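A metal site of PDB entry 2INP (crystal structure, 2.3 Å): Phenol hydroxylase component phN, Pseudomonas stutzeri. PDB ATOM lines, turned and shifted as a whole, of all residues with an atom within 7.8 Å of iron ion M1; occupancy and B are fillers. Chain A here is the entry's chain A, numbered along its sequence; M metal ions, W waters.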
ATOM      1  N   ILE A  99      33.816   7.757   3.120  1.00  0.00           N
ATOM      2  CA  ILE A  99      32.650   7.007   3.436  1.00  0.00           C
ATOM      3  C   ILE A  99      31.838   6.701   2.200  1.00  0.00           C
ATOM      4  O   ILE A  99      31.368   5.536   2.009  1.00  0.00           O
ATOM      5  CB  ILE A  99      31.761   7.773   4.411  1.00  0.00           C
ATOM      6  CG1 ILE A  99      32.236   7.742   5.868  1.00  0.00           C
ATOM      7  CG2 ILE A  99      30.274   7.199   4.449  1.00  0.00           C
ATOM      8  CD1 ILE A  99      33.672   7.300   6.276  1.00  0.00           C
ATOM      9  N   LEU A 102      32.766   3.859   0.231  1.00  0.00           N
ATOM     10  CA  LEU A 102      32.293   2.589   0.852  1.00  0.00           C
ATOM     11  C   LEU A 102      30.850   2.218   0.423  1.00  0.00           C
ATOM     12  O   LEU A 102      30.519   1.042   0.336  1.00  0.00           O
ATOM     13  CB  LEU A 102      32.382   2.676   2.375  1.00  0.00           C
ATOM     14  CG  LEU A 102      33.606   2.308   3.192  1.00  0.00           C
ATOM     15  CD1 LEU A 102      34.936   2.236   2.398  1.00  0.00           C
ATOM     16  CD2 LEU A 102      33.613   3.148   4.488  1.00  0.00           C
ATOM     17  N   GLU A 103      30.009   3.205   0.145  1.00  0.00           N
ATOM     18  CA  GLU A 103      28.661   2.938  -0.285  1.00  0.00           C
ATOM     19  C   GLU A 103      28.722   2.275  -1.647  1.00  0.00           C
ATOM     20  O   GLU A 103      27.934   1.380  -1.944  1.00  0.00           O
ATOM     21  CB  GLU A 103      27.885   4.254  -0.471  1.00  0.00           C
ATOM     22  CG  GLU A 103      27.719   5.185   0.723  1.00  0.00           C
ATOM     23  CD  GLU A 103      26.751   4.666   1.774  1.00  0.00           C
ATOM     24  OE1 GLU A 103      26.495   5.331   2.813  1.00  0.00           O
ATOM     25  OE2 GLU A 103      26.225   3.587   1.581  1.00  0.00           O
ATOM     26  N   HIS A 104      29.612   2.778  -2.518  1.00  0.00           N
ATOM     27  CA  HIS A 104      29.774   2.188  -3.841  1.00  0.00           C
ATOM     28  C   HIS A 104      30.379   0.787  -3.840  1.00  0.00           C
ATOM     29  O   HIS A 104      29.923  -0.054  -4.542  1.00  0.00           O
ATOM     30  CB  HIS A 104      30.520   3.142  -4.783  1.00  0.00           C
ATOM     31  CG  HIS A 104      30.096   3.002  -6.201  1.00  0.00           C
ATOM     32  ND1 HIS A 104      28.953   3.609  -6.706  1.00  0.00           N
ATOM     33  CD2 HIS A 104      30.602   2.246  -7.214  1.00  0.00           C
ATOM     34  CE1 HIS A 104      28.815   3.285  -7.986  1.00  0.00           C
ATOM     35  NE2 HIS A 104      29.797   2.450  -8.309  1.00  0.00           N
ATOM     36  N   ALA A 106      30.056  -1.362  -1.266  1.00  0.00           N
ATOM     37  CA  ALA A 106      28.905  -2.141  -0.780  1.00  0.00           C
ATOM     38  C   ALA A 106      27.881  -2.480  -1.877  1.00  0.00           C
ATOM     39  O   ALA A 106      27.435  -3.605  -1.955  1.00  0.00           O
ATOM     40  CB  ALA A 106      28.212  -1.460   0.486  1.00  0.00           C
ATOM     41  N   PHE A 107      27.506  -1.533  -2.711  1.00  0.00           N
ATOM     42  CA  PHE A 107      26.771  -1.797  -3.890  1.00  0.00           C
ATOM     43  C   PHE A 107      27.372  -2.976  -4.686  1.00  0.00           C
ATOM     44  O   PHE A 107      26.672  -3.894  -5.034  1.00  0.00           O
ATOM     45  CB  PHE A 107      26.692  -0.530  -4.778  1.00  0.00           C
ATOM     46  CG  PHE A 107      26.429  -0.847  -6.232  1.00  0.00           C
ATOM     47  CD1 PHE A 107      25.312  -1.594  -6.617  1.00  0.00           C
ATOM     48  CD2 PHE A 107      27.310  -0.419  -7.234  1.00  0.00           C
ATOM     49  CE1 PHE A 107      25.082  -1.916  -8.016  1.00  0.00           C
ATOM     50  CE2 PHE A 107      27.104  -0.745  -8.575  1.00  0.00           C
ATOM     51  CZ  PHE A 107      25.991  -1.489  -8.951  1.00  0.00           C
ATOM     52  N   TYR A 110      27.313  -6.449  -2.363  1.00  0.00           N
ATOM     53  CA  TYR A 110      25.990  -7.031  -2.266  1.00  0.00           C
ATOM     54  C   TYR A 110      25.460  -7.513  -3.588  1.00  0.00           C
ATOM     55  O   TYR A 110      24.593  -8.390  -3.601  1.00  0.00           O
ATOM     56  CB  TYR A 110      24.973  -6.050  -1.624  1.00  0.00           C
ATOM     57  CG  TYR A 110      25.113  -5.924  -0.133  1.00  0.00           C
ATOM     58  CD1 TYR A 110      25.851  -4.852   0.445  1.00  0.00           C
ATOM     59  CD2 TYR A 110      24.592  -6.890   0.699  1.00  0.00           C
ATOM     60  CE1 TYR A 110      26.085  -4.778   1.847  1.00  0.00           C
ATOM     61  CE2 TYR A 110      24.760  -6.824   2.096  1.00  0.00           C
ATOM     62  CZ  TYR A 110      25.527  -5.762   2.665  1.00  0.00           C
ATOM     63  OH  TYR A 110      25.692  -5.709   4.056  1.00  0.00           O
ATOM     64  N   GLN A 129      19.450  -4.616  -0.972  1.00  0.00           N
ATOM     65  CA  GLN A 129      20.548  -3.903  -0.291  1.00  0.00           C
ATOM     66  C   GLN A 129      21.510  -3.233  -1.271  1.00  0.00           C
ATOM     67  O   GLN A 129      21.792  -2.053  -1.143  1.00  0.00           O
ATOM     68  CB  GLN A 129      21.277  -4.837   0.643  1.00  0.00           C
ATOM     69  CG  GLN A 129      22.411  -4.114   1.307  1.00  0.00           C
ATOM     70  CD  GLN A 129      22.299  -3.925   2.792  1.00  0.00           C
ATOM     71  OE1 GLN A 129      21.495  -4.546   3.472  1.00  0.00           O
ATOM     72  NE2 GLN A 129      23.168  -3.111   3.313  1.00  0.00           N
ATOM     73  N   ASP A 132      20.153  -0.209  -3.030  1.00  0.00           N
ATOM     74  CA  ASP A 132      20.018   0.811  -1.996  1.00  0.00           C
ATOM     75  C   ASP A 132      21.341   1.526  -1.796  1.00  0.00           C
ATOM     76  O   ASP A 132      21.355   2.733  -1.690  1.00  0.00           O
ATOM     77  CB  ASP A 132      19.662   0.165  -0.641  1.00  0.00           C
ATOM     78  CG  ASP A 132      18.138  -0.090  -0.468  1.00  0.00           C
ATOM     79  OD1 ASP A 132      17.258   0.406  -1.260  1.00  0.00           O
ATOM     80  OD2 ASP A 132      17.843  -0.869   0.476  1.00  0.00           O
ATOM     81  N   GLU A 133      22.416   0.735  -1.679  1.00  0.00           N
ATOM     82  CA  GLU A 133      23.807   1.215  -1.585  1.00  0.00           C
ATOM     83  C   GLU A 133      24.177   2.077  -2.739  1.00  0.00           C
ATOM     84  O   GLU A 133      24.907   3.053  -2.554  1.00  0.00           O
ATOM     85  CB  GLU A 133      24.837   0.082  -1.407  1.00  0.00           C
ATOM     86  CG  GLU A 133      24.533  -0.803  -0.251  1.00  0.00           C
ATOM     87  CD  GLU A 133      24.487   0.008   1.075  1.00  0.00           C
ATOM     88  OE1 GLU A 133      24.288  -0.545   2.183  1.00  0.00           O
ATOM     89  OE2 GLU A 133      24.697   1.239   0.973  1.00  0.00           O
ATOM     90  N   LEU A 134      23.623   1.766  -3.899  1.00  0.00           N
ATOM     91  CA  LEU A 134      23.919   2.550  -5.079  1.00  0.00           C
ATOM     92  C   LEU A 134      23.160   3.892  -5.035  1.00  0.00           C
ATOM     93  O   LEU A 134      23.711   4.913  -5.394  1.00  0.00           O
ATOM     94  CB  LEU A 134      23.571   1.757  -6.363  1.00  0.00           C
ATOM     95  CG  LEU A 134      23.696   2.473  -7.700  1.00  0.00           C
ATOM     96  CD1 LEU A 134      25.170   2.876  -8.097  1.00  0.00           C
ATOM     97  CD2 LEU A 134      23.000   1.604  -8.833  1.00  0.00           C
ATOM     98  N   ARG A 135      21.888   3.854  -4.635  1.00  0.00           N
ATOM     99  CA  ARG A 135      21.179   5.050  -4.235  1.00  0.00           C
ATOM    100  C   ARG A 135      21.998   5.932  -3.278  1.00  0.00           C
ATOM    101  O   ARG A 135      22.147   7.082  -3.556  1.00  0.00           O
ATOM    102  CB  ARG A 135      19.892   4.731  -3.536  1.00  0.00           C
ATOM    103  CG  ARG A 135      19.194   6.037  -3.239  1.00  0.00           C
ATOM    104  CD  ARG A 135      17.814   5.852  -2.842  1.00  0.00           C
ATOM    105  NE  ARG A 135      17.698   6.065  -1.473  1.00  0.00           N
ATOM    106  CZ  ARG A 135      17.031   7.040  -0.848  1.00  0.00           C
ATOM    107  NH1 ARG A 135      16.281   7.976  -1.461  1.00  0.00           N
ATOM    108  NH2 ARG A 135      17.097   7.015   0.482  1.00  0.00           N
ATOM    109  N   HIS A 136      22.522   5.378  -2.170  1.00  0.00           N
ATOM    110  CA  HIS A 136      23.325   6.155  -1.255  1.00  0.00           C
ATOM    111  C   HIS A 136      24.548   6.777  -1.914  1.00  0.00           C
ATOM    112  O   HIS A 136      24.848   7.937  -1.664  1.00  0.00           O
ATOM    113  CB  HIS A 136      23.795   5.322  -0.079  1.00  0.00           C
ATOM    114  CG  HIS A 136      22.667   4.774   0.710  1.00  0.00           C
ATOM    115  ND1 HIS A 136      22.813   3.861   1.750  1.00  0.00           N
ATOM    116  CD2 HIS A 136      21.339   5.007   0.587  1.00  0.00           C
ATOM    117  CE1 HIS A 136      21.620   3.583   2.231  1.00  0.00           C
ATOM    118  NE2 HIS A 136      20.710   4.232   1.531  1.00  0.00           N
ATOM    119  N   SER A 137      25.248   5.976  -2.692  1.00  0.00           N
ATOM    120  CA  SER A 137      26.440   6.374  -3.408  1.00  0.00           C
ATOM    121  C   SER A 137      26.095   7.543  -4.318  1.00  0.00           C
ATOM    122  O   SER A 137      26.716   8.572  -4.293  1.00  0.00           O
ATOM    123  CB  SER A 137      26.987   5.213  -4.233  1.00  0.00           C
ATOM    124  OG  SER A 137      28.051   5.675  -5.050  1.00  0.00           O
ATOM    125  N   GLN A 140      24.637  10.812  -2.391  1.00  0.00           N
ATOM    126  CA  GLN A 140      25.743  11.553  -1.766  1.00  0.00           C
ATOM    127  C   GLN A 140      26.553  12.424  -2.743  1.00  0.00           C
ATOM    128  O   GLN A 140      26.948  13.526  -2.392  1.00  0.00           O
ATOM    129  CB  GLN A 140      26.684  10.585  -1.031  1.00  0.00           C
ATOM    130  CG  GLN A 140      25.911   9.964   0.149  1.00  0.00           C
ATOM    131  CD  GLN A 140      26.590   8.818   0.873  1.00  0.00           C
ATOM    132  OE1 GLN A 140      27.728   8.483   0.578  1.00  0.00           O
ATOM    133  NE2 GLN A 140      25.904   8.231   1.897  1.00  0.00           N
ATOM    134  N   PHE A 193      29.003  -3.958  10.587  1.00  0.00           N
ATOM    135  CA  PHE A 193      29.026  -2.574  10.137  1.00  0.00           C
ATOM    136  C   PHE A 193      27.605  -2.013  10.169  1.00  0.00           C
ATOM    137  O   PHE A 193      27.385  -0.955  10.758  1.00  0.00           O
ATOM    138  CB  PHE A 193      29.602  -2.582   8.714  1.00  0.00           C
ATOM    139  CG  PHE A 193      29.939  -1.224   8.134  1.00  0.00           C
ATOM    140  CD1 PHE A 193      31.024  -0.465   8.628  1.00  0.00           C
ATOM    141  CD2 PHE A 193      29.241  -0.749   6.996  1.00  0.00           C
ATOM    142  CE1 PHE A 193      31.412   0.765   8.008  1.00  0.00           C
ATOM    143  CE2 PHE A 193      29.595   0.497   6.374  1.00  0.00           C
ATOM    144  CZ  PHE A 193      30.705   1.240   6.874  1.00  0.00           C
ATOM    145  N   GLU A 194      26.625  -2.708   9.592  1.00  0.00           N
ATOM    146  CA  GLU A 194      25.275  -2.160   9.454  1.00  0.00           C
ATOM    147  C   GLU A 194      24.291  -2.383  10.583  1.00  0.00           C
ATOM    148  O   GLU A 194      23.188  -1.816  10.574  1.00  0.00           O
ATOM    149  CB  GLU A 194      24.659  -2.578   8.137  1.00  0.00           C
ATOM    150  CG  GLU A 194      25.438  -1.988   6.996  1.00  0.00           C
ATOM    151  CD  GLU A 194      24.618  -1.393   5.985  1.00  0.00           C
ATOM    152  OE1 GLU A 194      23.668  -1.987   5.512  1.00  0.00           O
ATOM    153  OE2 GLU A 194      24.889  -0.267   5.632  1.00  0.00           O
ATOM    154  N   LEU A 201      28.479   5.544  12.951  1.00  0.00           N
ATOM    155  CA  LEU A 201      28.759   6.247  11.700  1.00  0.00           C
ATOM    156  C   LEU A 201      27.590   7.214  11.281  1.00  0.00           C
ATOM    157  O   LEU A 201      27.778   8.414  11.018  1.00  0.00           O
ATOM    158  CB  LEU A 201      29.059   5.194  10.621  1.00  0.00           C
ATOM    159  CG  LEU A 201      29.146   5.695   9.182  1.00  0.00           C
ATOM    160  CD1 LEU A 201      30.146   6.837   9.110  1.00  0.00           C
ATOM    161  CD2 LEU A 201      29.534   4.562   8.157  1.00  0.00           C
ATOM    162  N   PHE A 202      26.382   6.684  11.238  1.00  0.00           N
ATOM    163  CA  PHE A 202      25.282   7.457  10.712  1.00  0.00           C
ATOM    164  C   PHE A 202      25.054   8.671  11.605  1.00  0.00           C
ATOM    165  O   PHE A 202      25.182   9.804  11.140  1.00  0.00           O
ATOM    166  CB  PHE A 202      24.016   6.584  10.647  1.00  0.00           C
ATOM    167  CG  PHE A 202      22.924   7.069   9.654  1.00  0.00           C
ATOM    168  CD1 PHE A 202      21.764   7.728  10.144  1.00  0.00           C
ATOM    169  CD2 PHE A 202      23.042   6.820   8.261  1.00  0.00           C
ATOM    170  CE1 PHE A 202      20.729   8.148   9.236  1.00  0.00           C
ATOM    171  CE2 PHE A 202      22.045   7.245   7.314  1.00  0.00           C
ATOM    172  CZ  PHE A 202      20.875   7.903   7.808  1.00  0.00           C
ATOM    173  N   PHE A 220      19.568  14.010   3.184  1.00  0.00           N
ATOM    174  CA  PHE A 220      19.921  12.685   2.674  1.00  0.00           C
ATOM    175  C   PHE A 220      19.764  11.666   3.843  1.00  0.00           C
ATOM    176  O   PHE A 220      19.288  10.527   3.636  1.00  0.00           O
ATOM    177  CB  PHE A 220      21.354  12.608   2.108  1.00  0.00           C
ATOM    178  CG  PHE A 220      21.881  11.199   2.154  1.00  0.00           C
ATOM    179  CD1 PHE A 220      21.431  10.208   1.169  1.00  0.00           C
ATOM    180  CD2 PHE A 220      22.716  10.782   3.209  1.00  0.00           C
ATOM    181  CE1 PHE A 220      21.834   8.872   1.233  1.00  0.00           C
ATOM    182  CE2 PHE A 220      23.127   9.365   3.315  1.00  0.00           C
ATOM    183  CZ  PHE A 220      22.704   8.414   2.319  1.00  0.00           C
ATOM    184  N   ALA A 224      17.273   8.255   3.960  1.00  0.00           N
ATOM    185  CA  ALA A 224      17.954   6.954   3.991  1.00  0.00           C
ATOM    186  C   ALA A 224      17.555   6.083   5.205  1.00  0.00           C
ATOM    187  O   ALA A 224      17.946   4.916   5.247  1.00  0.00           O
ATOM    188  CB  ALA A 224      19.563   7.157   4.077  1.00  0.00           C
ATOM    189  N   ASP A 227      15.806   2.903   4.555  1.00  0.00           N
ATOM    190  CA  ASP A 227      16.691   1.905   3.904  1.00  0.00           C
ATOM    191  C   ASP A 227      17.541   1.231   4.960  1.00  0.00           C
ATOM    192  O   ASP A 227      17.677   0.021   4.984  1.00  0.00           O
ATOM    193  CB  ASP A 227      17.691   2.552   2.937  1.00  0.00           C
ATOM    194  CG  ASP A 227      17.023   3.352   1.806  1.00  0.00           C
ATOM    195  OD1 ASP A 227      15.874   3.105   1.492  1.00  0.00           O
ATOM    196  OD2 ASP A 227      17.679   4.282   1.276  1.00  0.00           O
ATOM    197  N   GLU A 228      18.132   2.026   5.833  1.00  0.00           N
ATOM    198  CA  GLU A 228      18.937   1.443   6.858  1.00  0.00           C
ATOM    199  C   GLU A 228      18.107   0.532   7.809  1.00  0.00           C
ATOM    200  O   GLU A 228      18.641  -0.454   8.234  1.00  0.00           O
ATOM    201  CB  GLU A 228      19.753   2.481   7.604  1.00  0.00           C
ATOM    202  CG  GLU A 228      20.938   3.080   6.743  1.00  0.00           C
ATOM    203  CD  GLU A 228      21.790   2.033   5.986  1.00  0.00           C
ATOM    204  OE1 GLU A 228      22.301   0.996   6.512  1.00  0.00           O
ATOM    205  OE2 GLU A 228      21.989   2.284   4.786  1.00  0.00           O
ATOM    206  N   HIS A 231      18.295  -2.735   6.182  1.00  0.00           N
ATOM    207  CA  HIS A 231      19.628  -3.287   6.227  1.00  0.00           C
ATOM    208  C   HIS A 231      19.995  -3.798   7.587  1.00  0.00           C
ATOM    209  O   HIS A 231      20.772  -4.721   7.683  1.00  0.00           O
ATOM    210  CB  HIS A 231      20.643  -2.207   5.766  1.00  0.00           C
ATOM    211  CG  HIS A 231      20.293  -1.618   4.422  1.00  0.00           C
ATOM    212  ND1 HIS A 231      20.853  -0.462   3.933  1.00  0.00           N
ATOM    213  CD2 HIS A 231      19.428  -2.033   3.450  1.00  0.00           C
ATOM    214  CE1 HIS A 231      20.370  -0.185   2.731  1.00  0.00           C
ATOM    215  NE2 HIS A 231      19.493  -1.113   2.425  1.00  0.00           N
HETATM  216 FE    FE M   1      24.581   2.696   2.654  1.00  0.00          FE
HETATM  217 FE    FE M   2      23.064   0.488   4.600  1.00  0.00          FE
HETATM  218  O   HOH W   1      24.677   5.006   4.252  1.00  0.00           O
HETATM  219  O   HOH W   2      26.113   1.892   3.495  1.00  0.00           O
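Residues that only touch iron ion M1: Glu 228 (3.4 Å). The nearest printed residue that does not touch iron ion M1 is Glu 194 (4.2 Å).
Iron ion M1 is bound by water W2 (1.9 Å). OE2 of Glu 103 binds iron ion M1 (2.2 Å). The side-chain carboxylate (OE2) of Glu 133 is bound to iron ion M1 (2.2 Å). Iron ion M1 is bound by a ring nitrogen (ND1) of His 136 (2.3 Å). Iron ion M1 has four donor atoms within binding distance. Slightly farther from iron ion M1 lies water W1 (2.8 Å).
NE2 of Gln 140 sits at hydrogen-bond distance from OE1 of Glu 103 (3.1 Å). The side-chain carboxylate (OE1) of Glu 133 sits at hydrogen-bond distance from the side-chain amide nitrogen (NE2) of Gln 129 (3.0 Å). The side-chain carboxylate of Asp 227 sits at hydrogen-bond distance from a ring nitrogen (NE2) of His 136 (3.0 Å).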
